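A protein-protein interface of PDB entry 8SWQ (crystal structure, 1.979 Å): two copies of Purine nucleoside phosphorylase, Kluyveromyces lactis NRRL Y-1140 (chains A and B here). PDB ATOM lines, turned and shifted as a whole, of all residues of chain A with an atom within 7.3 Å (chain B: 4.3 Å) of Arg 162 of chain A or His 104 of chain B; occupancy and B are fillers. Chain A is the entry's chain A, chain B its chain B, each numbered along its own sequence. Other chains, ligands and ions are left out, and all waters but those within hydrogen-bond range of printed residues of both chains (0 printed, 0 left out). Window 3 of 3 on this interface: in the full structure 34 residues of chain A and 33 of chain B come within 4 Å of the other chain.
Hydrophobic or aromatic side chains of chain B within 4 Å of the printed part of chain A: His 210. Printed residues of chain A that touch a printed residue of chain B: Gly 157, Arg 162, Gly 163, Ala 164 and Arg 172. Among the printed residues, 10 pairs touch across the chains.
No position is printed for both chains. Of the 10 pairs that touch across the chains among the printed residues, none has its exchanged pair printed and touching as well.
The guanidinium group (NE) of Arg 162 of chain A sits at hydrogen-bond distance from a ring nitrogen (NE2) of His 210 of chain B (3.1 Å). The backbone carbonyl oxygen (O) of His 104 of chain B lies within hydrogen-bond range of the guanidinium group (NH2) of Arg 162 of chain A, at 3.1 Å. N of Gly 163 of chain A lies within hydrogen-bond range of O of Tyr 101 of chain B, 2.8 Å away. NE of Arg 162 of chain A sits at hydrogen-bond distance from O of Ser 100 of chain B.
The guanidinium group (NH2) of Arg 172 of chain A sits at hydrogen-bond distance from the backbone carbonyl oxygen (O) of Gly 163 of chain A (2.8 Å). The side-chain carboxylate (OE1) of Glu 102 of chain B is in hydrogen-bond range of a ring nitrogen (ND1) of His 99 of chain B (3.0 Å). The backbone carbonyl oxygen (O) of Leu 161 of chain A sits at hydrogen-bond distance from the guanidinium group (NH1) of Arg 172 of chain A (3.1 Å). OG of Ser 100 of chain B sits at hydrogen-bond distance from NE2 of His 210 of chain B (3.1 Å). NE2 of His 104 of chain B is in hydrogen-bond range of OE2 of Glu 102 of chain B, 3.4 Å away. OH of Tyr 101 of chain B sits at hydrogen-bond distance from ND1 of His 99 of chain B, at 3.4 Å.
Printed residues of chain B within 4 Å of Arg 162 of chain A: Ser 100 (3.2 Å), Tyr 101 (3.5 Å), His 104 (3.1 Å) and His 210 (3.1 Å). Of the printed residues of chain B, Gly 163 of chain A touches Tyr 101, Glu 102 and Gly 103. Printed residues of chain A within 4 Å of Tyr 101 of chain B: Arg 162, Gly 163 and Arg 172. Printed residues of chain A within 4 Å of Gly 103 of chain B: Gly 163. Of chain A, only Arg 162 (3.1 Å) comes within 4 Å of His 104 of chain B. Of the printed residues of chain A, His 210 of chain B touches Gly 157 (3.7 Å) and Arg 162 (3.1 Å).
CG of His 210 of chain B touches CA of Gly 157 of chain A, at 3.7 Å. Tyr 101 of chain B touches Arg 162 of chain A (O to CA, 3.5 Å). Gly 163 of chain A touches Glu 102 of chain B (C to O, 3.4 Å). Gly 163 of chain A touches Gly 103 of chain B (N to N, 3.8 Å). N of Ala 164 of chain A touches O of Glu 102 of chain B, at 3.6 Å. Tyr 101 of chain B touches Arg 172 of chain A.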
ATOM      1  N   GLN A  10       8.924  22.415  34.155  1.00  0.00           N
ATOM      2  CA  GLN A  10      10.127  21.928  34.818  1.00  0.00           C
ATOM      3  C   GLN A  10      11.069  23.086  35.144  1.00  0.00           C
ATOM      4  O   GLN A  10      11.662  23.127  36.226  1.00  0.00           O
ATOM      5  CB  GLN A  10      10.837  20.873  33.957  1.00  0.00           C
ATOM      6  CG  GLN A  10      10.213  19.482  34.007  1.00  0.00           C
ATOM      7  CD  GLN A  10      11.052  18.430  33.285  1.00  0.00           C
ATOM      8  OE1 GLN A  10      12.205  18.179  33.648  1.00  0.00           O
ATOM      9  NE2 GLN A  10      10.472  17.811  32.255  1.00  0.00           N
ATOM     10  N   ALA A 107      13.688  12.158  35.789  1.00  0.00           N
ATOM     11  CA  ALA A 107      13.729  13.621  35.875  1.00  0.00           C
ATOM     12  C   ALA A 107      13.595  14.116  37.316  1.00  0.00           C
ATOM     13  O   ALA A 107      14.286  15.056  37.735  1.00  0.00           O
ATOM     14  CB  ALA A 107      12.643  14.238  35.004  1.00  0.00           C
ATOM     15  N   GLY A 157      15.299   3.349  26.540  1.00  0.00           N
ATOM     16  CA  GLY A 157      14.180   4.275  26.592  1.00  0.00           C
ATOM     17  C   GLY A 157      13.898   4.992  27.900  1.00  0.00           C
ATOM     18  O   GLY A 157      12.964   5.778  27.975  1.00  0.00           O
ATOM     19  N   PHE A 158      14.686   4.715  28.935  1.00  0.00           N
ATOM     20  CA  PHE A 158      14.523   5.369  30.241  1.00  0.00           C
ATOM     21  C   PHE A 158      15.757   6.201  30.511  1.00  0.00           C
ATOM     22  O   PHE A 158      16.748   5.697  31.039  1.00  0.00           O
ATOM     23  CB  PHE A 158      14.369   4.319  31.348  1.00  0.00           C
ATOM     24  CG  PHE A 158      13.139   3.471  31.199  1.00  0.00           C
ATOM     25  CD1 PHE A 158      13.169   2.302  30.455  1.00  0.00           C
ATOM     26  CD2 PHE A 158      11.951   3.846  31.807  1.00  0.00           C
ATOM     27  CE1 PHE A 158      12.024   1.516  30.310  1.00  0.00           C
ATOM     28  CE2 PHE A 158      10.798   3.063  31.678  1.00  0.00           C
ATOM     29  CZ  PHE A 158      10.839   1.899  30.928  1.00  0.00           C
ATOM     30  N   HIS A 159      15.698   7.480  30.164  1.00  0.00           N
ATOM     31  CA  HIS A 159      16.900   8.319  30.149  1.00  0.00           C
ATOM     32  C   HIS A 159      16.562   9.659  30.803  1.00  0.00           C
ATOM     33  O   HIS A 159      15.502  10.238  30.529  1.00  0.00           O
ATOM     34  CB  HIS A 159      17.332   8.539  28.687  1.00  0.00           C
ATOM     35  CG  HIS A 159      18.728   9.059  28.531  1.00  0.00           C
ATOM     36  ND1 HIS A 159      19.103  10.314  28.964  1.00  0.00           N
ATOM     37  CD2 HIS A 159      19.839   8.495  27.994  1.00  0.00           C
ATOM     38  CE1 HIS A 159      20.393  10.498  28.706  1.00  0.00           C
ATOM     39  NE2 HIS A 159      20.859   9.410  28.117  1.00  0.00           N
ATOM     40  N   PRO A 160      17.451  10.169  31.669  1.00  0.00           N
ATOM     41  CA  PRO A 160      17.099  11.428  32.343  1.00  0.00           C
ATOM     42  C   PRO A 160      17.084  12.652  31.420  1.00  0.00           C
ATOM     43  O   PRO A 160      16.491  13.673  31.783  1.00  0.00           O
ATOM     44  CB  PRO A 160      18.188  11.572  33.422  1.00  0.00           C
ATOM     45  CG  PRO A 160      19.369  10.827  32.856  1.00  0.00           C
ATOM     46  CD  PRO A 160      18.743   9.628  32.136  1.00  0.00           C
ATOM     47  N   LEU A 161      17.695  12.571  30.240  1.00  0.00           N
ATOM     48  CA  LEU A 161      17.687  13.744  29.349  1.00  0.00           C
ATOM     49  C   LEU A 161      16.574  13.689  28.300  1.00  0.00           C
ATOM     50  O   LEU A 161      16.459  14.588  27.460  1.00  0.00           O
ATOM     51  CB  LEU A 161      19.049  13.939  28.670  1.00  0.00           C
ATOM     52  CG  LEU A 161      20.256  14.067  29.593  1.00  0.00           C
ATOM     53  CD1 LEU A 161      21.544  14.214  28.765  1.00  0.00           C
ATOM     54  CD2 LEU A 161      20.092  15.260  30.536  1.00  0.00           C
ATOM     55  N   ARG A 162      15.747  12.650  28.331  1.00  0.00           N
ATOM     56  CA  ARG A 162      14.606  12.584  27.391  1.00  0.00           C
ATOM     57  C   ARG A 162      13.692  13.807  27.550  1.00  0.00           C
ATOM     58  O   ARG A 162      13.414  14.229  28.670  1.00  0.00           O
ATOM     59  CB  ARG A 162      13.789  11.312  27.616  1.00  0.00           C
ATOM     60  CG  ARG A 162      12.566  11.182  26.698  1.00  0.00           C
ATOM     61  CD  ARG A 162      11.906   9.819  26.829  1.00  0.00           C
ATOM     62  NE  ARG A 162      11.122   9.514  25.630  1.00  0.00           N
ATOM     63  CZ  ARG A 162       9.798   9.484  25.598  1.00  0.00           C
ATOM     64  NH1 ARG A 162       9.115   9.721  26.708  1.00  0.00           N
ATOM     65  NH2 ARG A 162       9.160   9.211  24.466  1.00  0.00           N
ATOM     66  N   GLY A 163      13.249  14.382  26.432  1.00  0.00           N
ATOM     67  CA  GLY A 163      12.386  15.547  26.457  1.00  0.00           C
ATOM     68  C   GLY A 163      13.085  16.716  25.790  1.00  0.00           C
ATOM     69  O   GLY A 163      14.205  16.575  25.290  1.00  0.00           O
ATOM     70  N   ALA A 164      12.436  17.873  25.777  1.00  0.00           N
ATOM     71  CA  ALA A 164      13.076  19.067  25.251  1.00  0.00           C
ATOM     72  C   ALA A 164      14.361  19.287  26.056  1.00  0.00           C
ATOM     73  O   ALA A 164      14.423  18.977  27.250  1.00  0.00           O
ATOM     74  CB  ALA A 164      12.150  20.276  25.370  1.00  0.00           C
ATOM     75  N   ASN A 165      15.389  19.805  25.397  1.00  0.00           N
ATOM     76  CA  ASN A 165      16.680  20.019  26.034  1.00  0.00           C
ATOM     77  C   ASN A 165      16.692  21.304  26.857  1.00  0.00           C
ATOM     78  O   ASN A 165      16.118  22.317  26.444  1.00  0.00           O
ATOM     79  CB  ASN A 165      17.778  20.098  24.964  1.00  0.00           C
ATOM     80  CG  ASN A 165      19.151  20.298  25.564  1.00  0.00           C
ATOM     81  OD1 ASN A 165      19.621  19.456  26.319  1.00  0.00           O
ATOM     82  ND2 ASN A 165      19.809  21.406  25.225  1.00  0.00           N
ATOM     83  N   PHE A 166      17.347  21.281  28.016  1.00  0.00           N
ATOM     84  CA  PHE A 166      17.590  22.533  28.743  1.00  0.00           C
ATOM     85  C   PHE A 166      18.777  23.249  28.133  1.00  0.00           C
ATOM     86  O   PHE A 166      19.901  23.112  28.615  1.00  0.00           O
ATOM     87  CB  PHE A 166      17.858  22.267  30.231  1.00  0.00           C
ATOM     88  CG  PHE A 166      16.645  21.801  30.985  1.00  0.00           C
ATOM     89  CD1 PHE A 166      15.764  22.722  31.551  1.00  0.00           C
ATOM     90  CD2 PHE A 166      16.374  20.448  31.113  1.00  0.00           C
ATOM     91  CE1 PHE A 166      14.630  22.292  32.240  1.00  0.00           C
ATOM     92  CE2 PHE A 166      15.242  20.004  31.797  1.00  0.00           C
ATOM     93  CZ  PHE A 166      14.371  20.928  32.366  1.00  0.00           C
ATOM     94  N   ARG A 172      22.268  19.471  23.422  1.00  0.00           N
ATOM     95  CA  ARG A 172      21.230  18.492  23.116  1.00  0.00           C
ATOM     96  C   ARG A 172      21.830  17.089  23.095  1.00  0.00           C
ATOM     97  O   ARG A 172      21.188  16.125  23.529  1.00  0.00           O
ATOM     98  CB  ARG A 172      20.563  18.836  21.773  1.00  0.00           C
ATOM     99  CG  ARG A 172      19.770  17.684  21.127  1.00  0.00           C
ATOM    100  CD  ARG A 172      18.346  17.483  21.691  1.00  0.00           C
ATOM    101  NE  ARG A 172      18.341  16.873  23.025  1.00  0.00           N
ATOM    102  CZ  ARG A 172      17.233  16.572  23.699  1.00  0.00           C
ATOM    103  NH1 ARG A 172      17.305  16.030  24.907  1.00  0.00           N
ATOM    104  NH2 ARG A 172      16.044  16.812  23.156  1.00  0.00           N
ATOM    105  N   LYS B  70       4.120  16.677  14.609  1.00  0.00           N
ATOM    106  CA  LYS B  70       4.772  17.392  15.709  1.00  0.00           C
ATOM    107  C   LYS B  70       5.935  18.262  15.231  1.00  0.00           C
ATOM    108  O   LYS B  70       6.591  17.944  14.239  1.00  0.00           O
ATOM    109  CB  LYS B  70       5.257  16.418  16.793  1.00  0.00           C
ATOM    110  CG  LYS B  70       4.151  15.622  17.475  1.00  0.00           C
ATOM    111  CD  LYS B  70       2.904  16.471  17.663  1.00  0.00           C
ATOM    112  CE  LYS B  70       1.972  15.884  18.710  1.00  0.00           C
ATOM    113  NZ  LYS B  70       0.678  16.631  18.760  1.00  0.00           N
ATOM    114  N   LEU B  98      11.245  12.906  13.409  1.00  0.00           N
ATOM    115  CA  LEU B  98      11.098  13.138  14.846  1.00  0.00           C
ATOM    116  C   LEU B  98      11.820  12.012  15.571  1.00  0.00           C
ATOM    117  O   LEU B  98      11.966  10.916  15.034  1.00  0.00           O
ATOM    118  CB  LEU B  98       9.621  13.166  15.262  1.00  0.00           C
ATOM    119  CG  LEU B  98       8.690  14.254  14.725  1.00  0.00           C
ATOM    120  CD1 LEU B  98       9.441  15.547  14.411  1.00  0.00           C
ATOM    121  CD2 LEU B  98       7.906  13.761  13.510  1.00  0.00           C
ATOM    122  N   HIS B  99      12.309  12.285  16.771  1.00  0.00           N
ATOM    123  CA  HIS B  99      13.050  11.274  17.518  1.00  0.00           C
ATOM    124  C   HIS B  99      12.416  11.107  18.878  1.00  0.00           C
ATOM    125  O   HIS B  99      11.982  12.083  19.489  1.00  0.00           O
ATOM    126  CB  HIS B  99      14.490  11.708  17.742  1.00  0.00           C
ATOM    127  CG  HIS B  99      15.264  11.969  16.486  1.00  0.00           C
ATOM    128  ND1 HIS B  99      15.183  13.160  15.794  1.00  0.00           N
ATOM    129  CD2 HIS B  99      16.169  11.210  15.822  1.00  0.00           C
ATOM    130  CE1 HIS B  99      15.994  13.118  14.748  1.00  0.00           C
ATOM    131  NE2 HIS B  99      16.604  11.945  14.744  1.00  0.00           N
ATOM    132  N   SER B 100      12.398   9.885  19.382  1.00  0.00           N
ATOM    133  CA  SER B 100      11.850   9.662  20.709  1.00  0.00           C
ATOM    134  C   SER B 100      12.603  10.405  21.817  1.00  0.00           C
ATOM    135  O   SER B 100      12.004  10.756  22.833  1.00  0.00           O
ATOM    136  CB  SER B 100      11.780   8.163  21.023  1.00  0.00           C
ATOM    137  OG  SER B 100      11.304   7.968  22.350  1.00  0.00           O
ATOM    138  N   TYR B 101      13.900  10.673  21.644  1.00  0.00           N
ATOM    139  CA  TYR B 101      14.610  11.393  22.713  1.00  0.00           C
ATOM    140  C   TYR B 101      14.064  12.808  22.930  1.00  0.00           C
ATOM    141  O   TYR B 101      14.319  13.440  23.968  1.00  0.00           O
ATOM    142  CB  TYR B 101      16.143  11.436  22.505  1.00  0.00           C
ATOM    143  CG  TYR B 101      16.613  12.070  21.209  1.00  0.00           C
ATOM    144  CD1 TYR B 101      16.497  13.441  20.987  1.00  0.00           C
ATOM    145  CD2 TYR B 101      17.185  11.297  20.216  1.00  0.00           C
ATOM    146  CE1 TYR B 101      16.931  14.016  19.789  1.00  0.00           C
ATOM    147  CE2 TYR B 101      17.622  11.857  19.029  1.00  0.00           C
ATOM    148  CZ  TYR B 101      17.499  13.206  18.821  1.00  0.00           C
ATOM    149  OH  TYR B 101      17.932  13.732  17.623  1.00  0.00           O
ATOM    150  N   GLU B 102      13.327  13.312  21.947  1.00  0.00           N
ATOM    151  CA  GLU B 102      12.789  14.670  22.032  1.00  0.00           C
ATOM    152  C   GLU B 102      11.566  14.705  22.936  1.00  0.00           C
ATOM    153  O   GLU B 102      11.033  15.773  23.225  1.00  0.00           O
ATOM    154  CB  GLU B 102      12.403  15.198  20.641  1.00  0.00           C
ATOM    155  CG  GLU B 102      13.531  15.259  19.606  1.00  0.00           C
ATOM    156  CD  GLU B 102      13.029  15.727  18.233  1.00  0.00           C
ATOM    157  OE1 GLU B 102      13.389  15.111  17.195  1.00  0.00           O
ATOM    158  OE2 GLU B 102      12.269  16.720  18.193  1.00  0.00           O
ATOM    159  N   GLY B 103      11.108  13.536  23.375  1.00  0.00           N
ATOM    160  CA  GLY B 103       9.925  13.470  24.216  1.00  0.00           C
ATOM    161  C   GLY B 103       8.664  13.070  23.462  1.00  0.00           C
ATOM    162  O   GLY B 103       7.576  13.011  24.038  1.00  0.00           O
ATOM    163  N   HIS B 104       8.799  12.802  22.168  1.00  0.00           N
ATOM    164  CA  HIS B 104       7.649  12.398  21.363  1.00  0.00           C
ATOM    165  C   HIS B 104       7.447  10.901  21.530  1.00  0.00           C
ATOM    166  O   HIS B 104       8.417  10.154  21.572  1.00  0.00           O
ATOM    167  CB  HIS B 104       7.888  12.696  19.882  1.00  0.00           C
ATOM    168  CG  HIS B 104       8.217  14.128  19.599  1.00  0.00           C
ATOM    169  ND1 HIS B 104       7.412  15.171  20.001  1.00  0.00           N
ATOM    170  CD2 HIS B 104       9.265  14.690  18.949  1.00  0.00           C
ATOM    171  CE1 HIS B 104       7.949  16.314  19.614  1.00  0.00           C
ATOM    172  NE2 HIS B 104       9.076  16.051  18.977  1.00  0.00           N
ATOM    173  N   SER B 105       6.196  10.463  21.610  1.00  0.00           N
ATOM    174  CA  SER B 105       5.899   9.031  21.611  1.00  0.00           C
ATOM    175  C   SER B 105       6.299   8.435  20.263  1.00  0.00           C
ATOM    176  O   SER B 105       6.331   9.143  19.250  1.00  0.00           O
ATOM    177  CB  SER B 105       4.407   8.796  21.852  1.00  0.00           C
ATOM    178  OG  SER B 105       3.653   9.192  20.718  1.00  0.00           O
ATOM    179  N   LEU B 106       6.606   7.140  20.242  1.00  0.00           N
ATOM    180  CA  LEU B 106       6.946   6.484  18.986  1.00  0.00           C
ATOM    181  C   LEU B 106       5.804   6.598  17.967  1.00  0.00           C
ATOM    182  O   LEU B 106       6.053   6.718  16.768  1.00  0.00           O
ATOM    183  CB  LEU B 106       7.373   5.028  19.212  1.00  0.00           C
ATOM    184  CG  LEU B 106       8.796   4.879  19.759  1.00  0.00           C
ATOM    185  CD1 LEU B 106       9.191   3.413  19.834  1.00  0.00           C
ATOM    186  CD2 LEU B 106       9.789   5.645  18.897  1.00  0.00           C
ATOM    187  N   GLU B 108       3.748   9.175  17.589  1.00  0.00           N
ATOM    188  CA  GLU B 108       3.891  10.513  17.001  1.00  0.00           C
ATOM    189  C   GLU B 108       5.032  10.568  15.990  1.00  0.00           C
ATOM    190  O   GLU B 108       4.948  11.275  14.983  1.00  0.00           O
ATOM    191  CB  GLU B 108       4.108  11.572  18.104  1.00  0.00           C
ATOM    192  CG  GLU B 108       2.882  11.787  18.996  1.00  0.00           C
ATOM    193  CD  GLU B 108       3.202  12.463  20.329  1.00  0.00           C
ATOM    194  OE1 GLU B 108       4.384  12.468  20.752  1.00  0.00           O
ATOM    195  OE2 GLU B 108       2.255  12.982  20.964  1.00  0.00           O
ATOM    196  N   THR B 109       6.106   9.825  16.237  1.00  0.00           N
ATOM    197  CA  THR B 109       7.218   9.875  15.292  1.00  0.00           C
ATOM    198  C   THR B 109       6.897   9.177  13.967  1.00  0.00           C
ATOM    199  O   THR B 109       7.529   9.463  12.958  1.00  0.00           O
ATOM    200  CB  THR B 109       8.551   9.348  15.877  1.00  0.00           C
ATOM    201  OG1 THR B 109       8.523   7.920  15.961  1.00  0.00           O
ATOM    202  CG2 THR B 109       8.803   9.949  17.244  1.00  0.00           C
ATOM    203  N   HIS B 210      17.955   4.742  22.412  1.00  0.00           N
ATOM    204  CA  HIS B 210      17.079   5.879  22.619  1.00  0.00           C
ATOM    205  C   HIS B 210      17.779   7.252  22.542  1.00  0.00           C
ATOM    206  O   HIS B 210      17.220   8.205  21.983  1.00  0.00           O
ATOM    207  CB  HIS B 210      16.315   5.703  23.931  1.00  0.00           C
ATOM    208  CG  HIS B 210      15.327   6.787  24.201  1.00  0.00           C
ATOM    209  ND1 HIS B 210      15.639   7.901  24.950  1.00  0.00           N
ATOM    210  CD2 HIS B 210      14.031   6.926  23.837  1.00  0.00           C
ATOM    211  CE1 HIS B 210      14.576   8.684  25.033  1.00  0.00           C
ATOM    212  NE2 HIS B 210      13.588   8.114  24.367  1.00  0.00           N
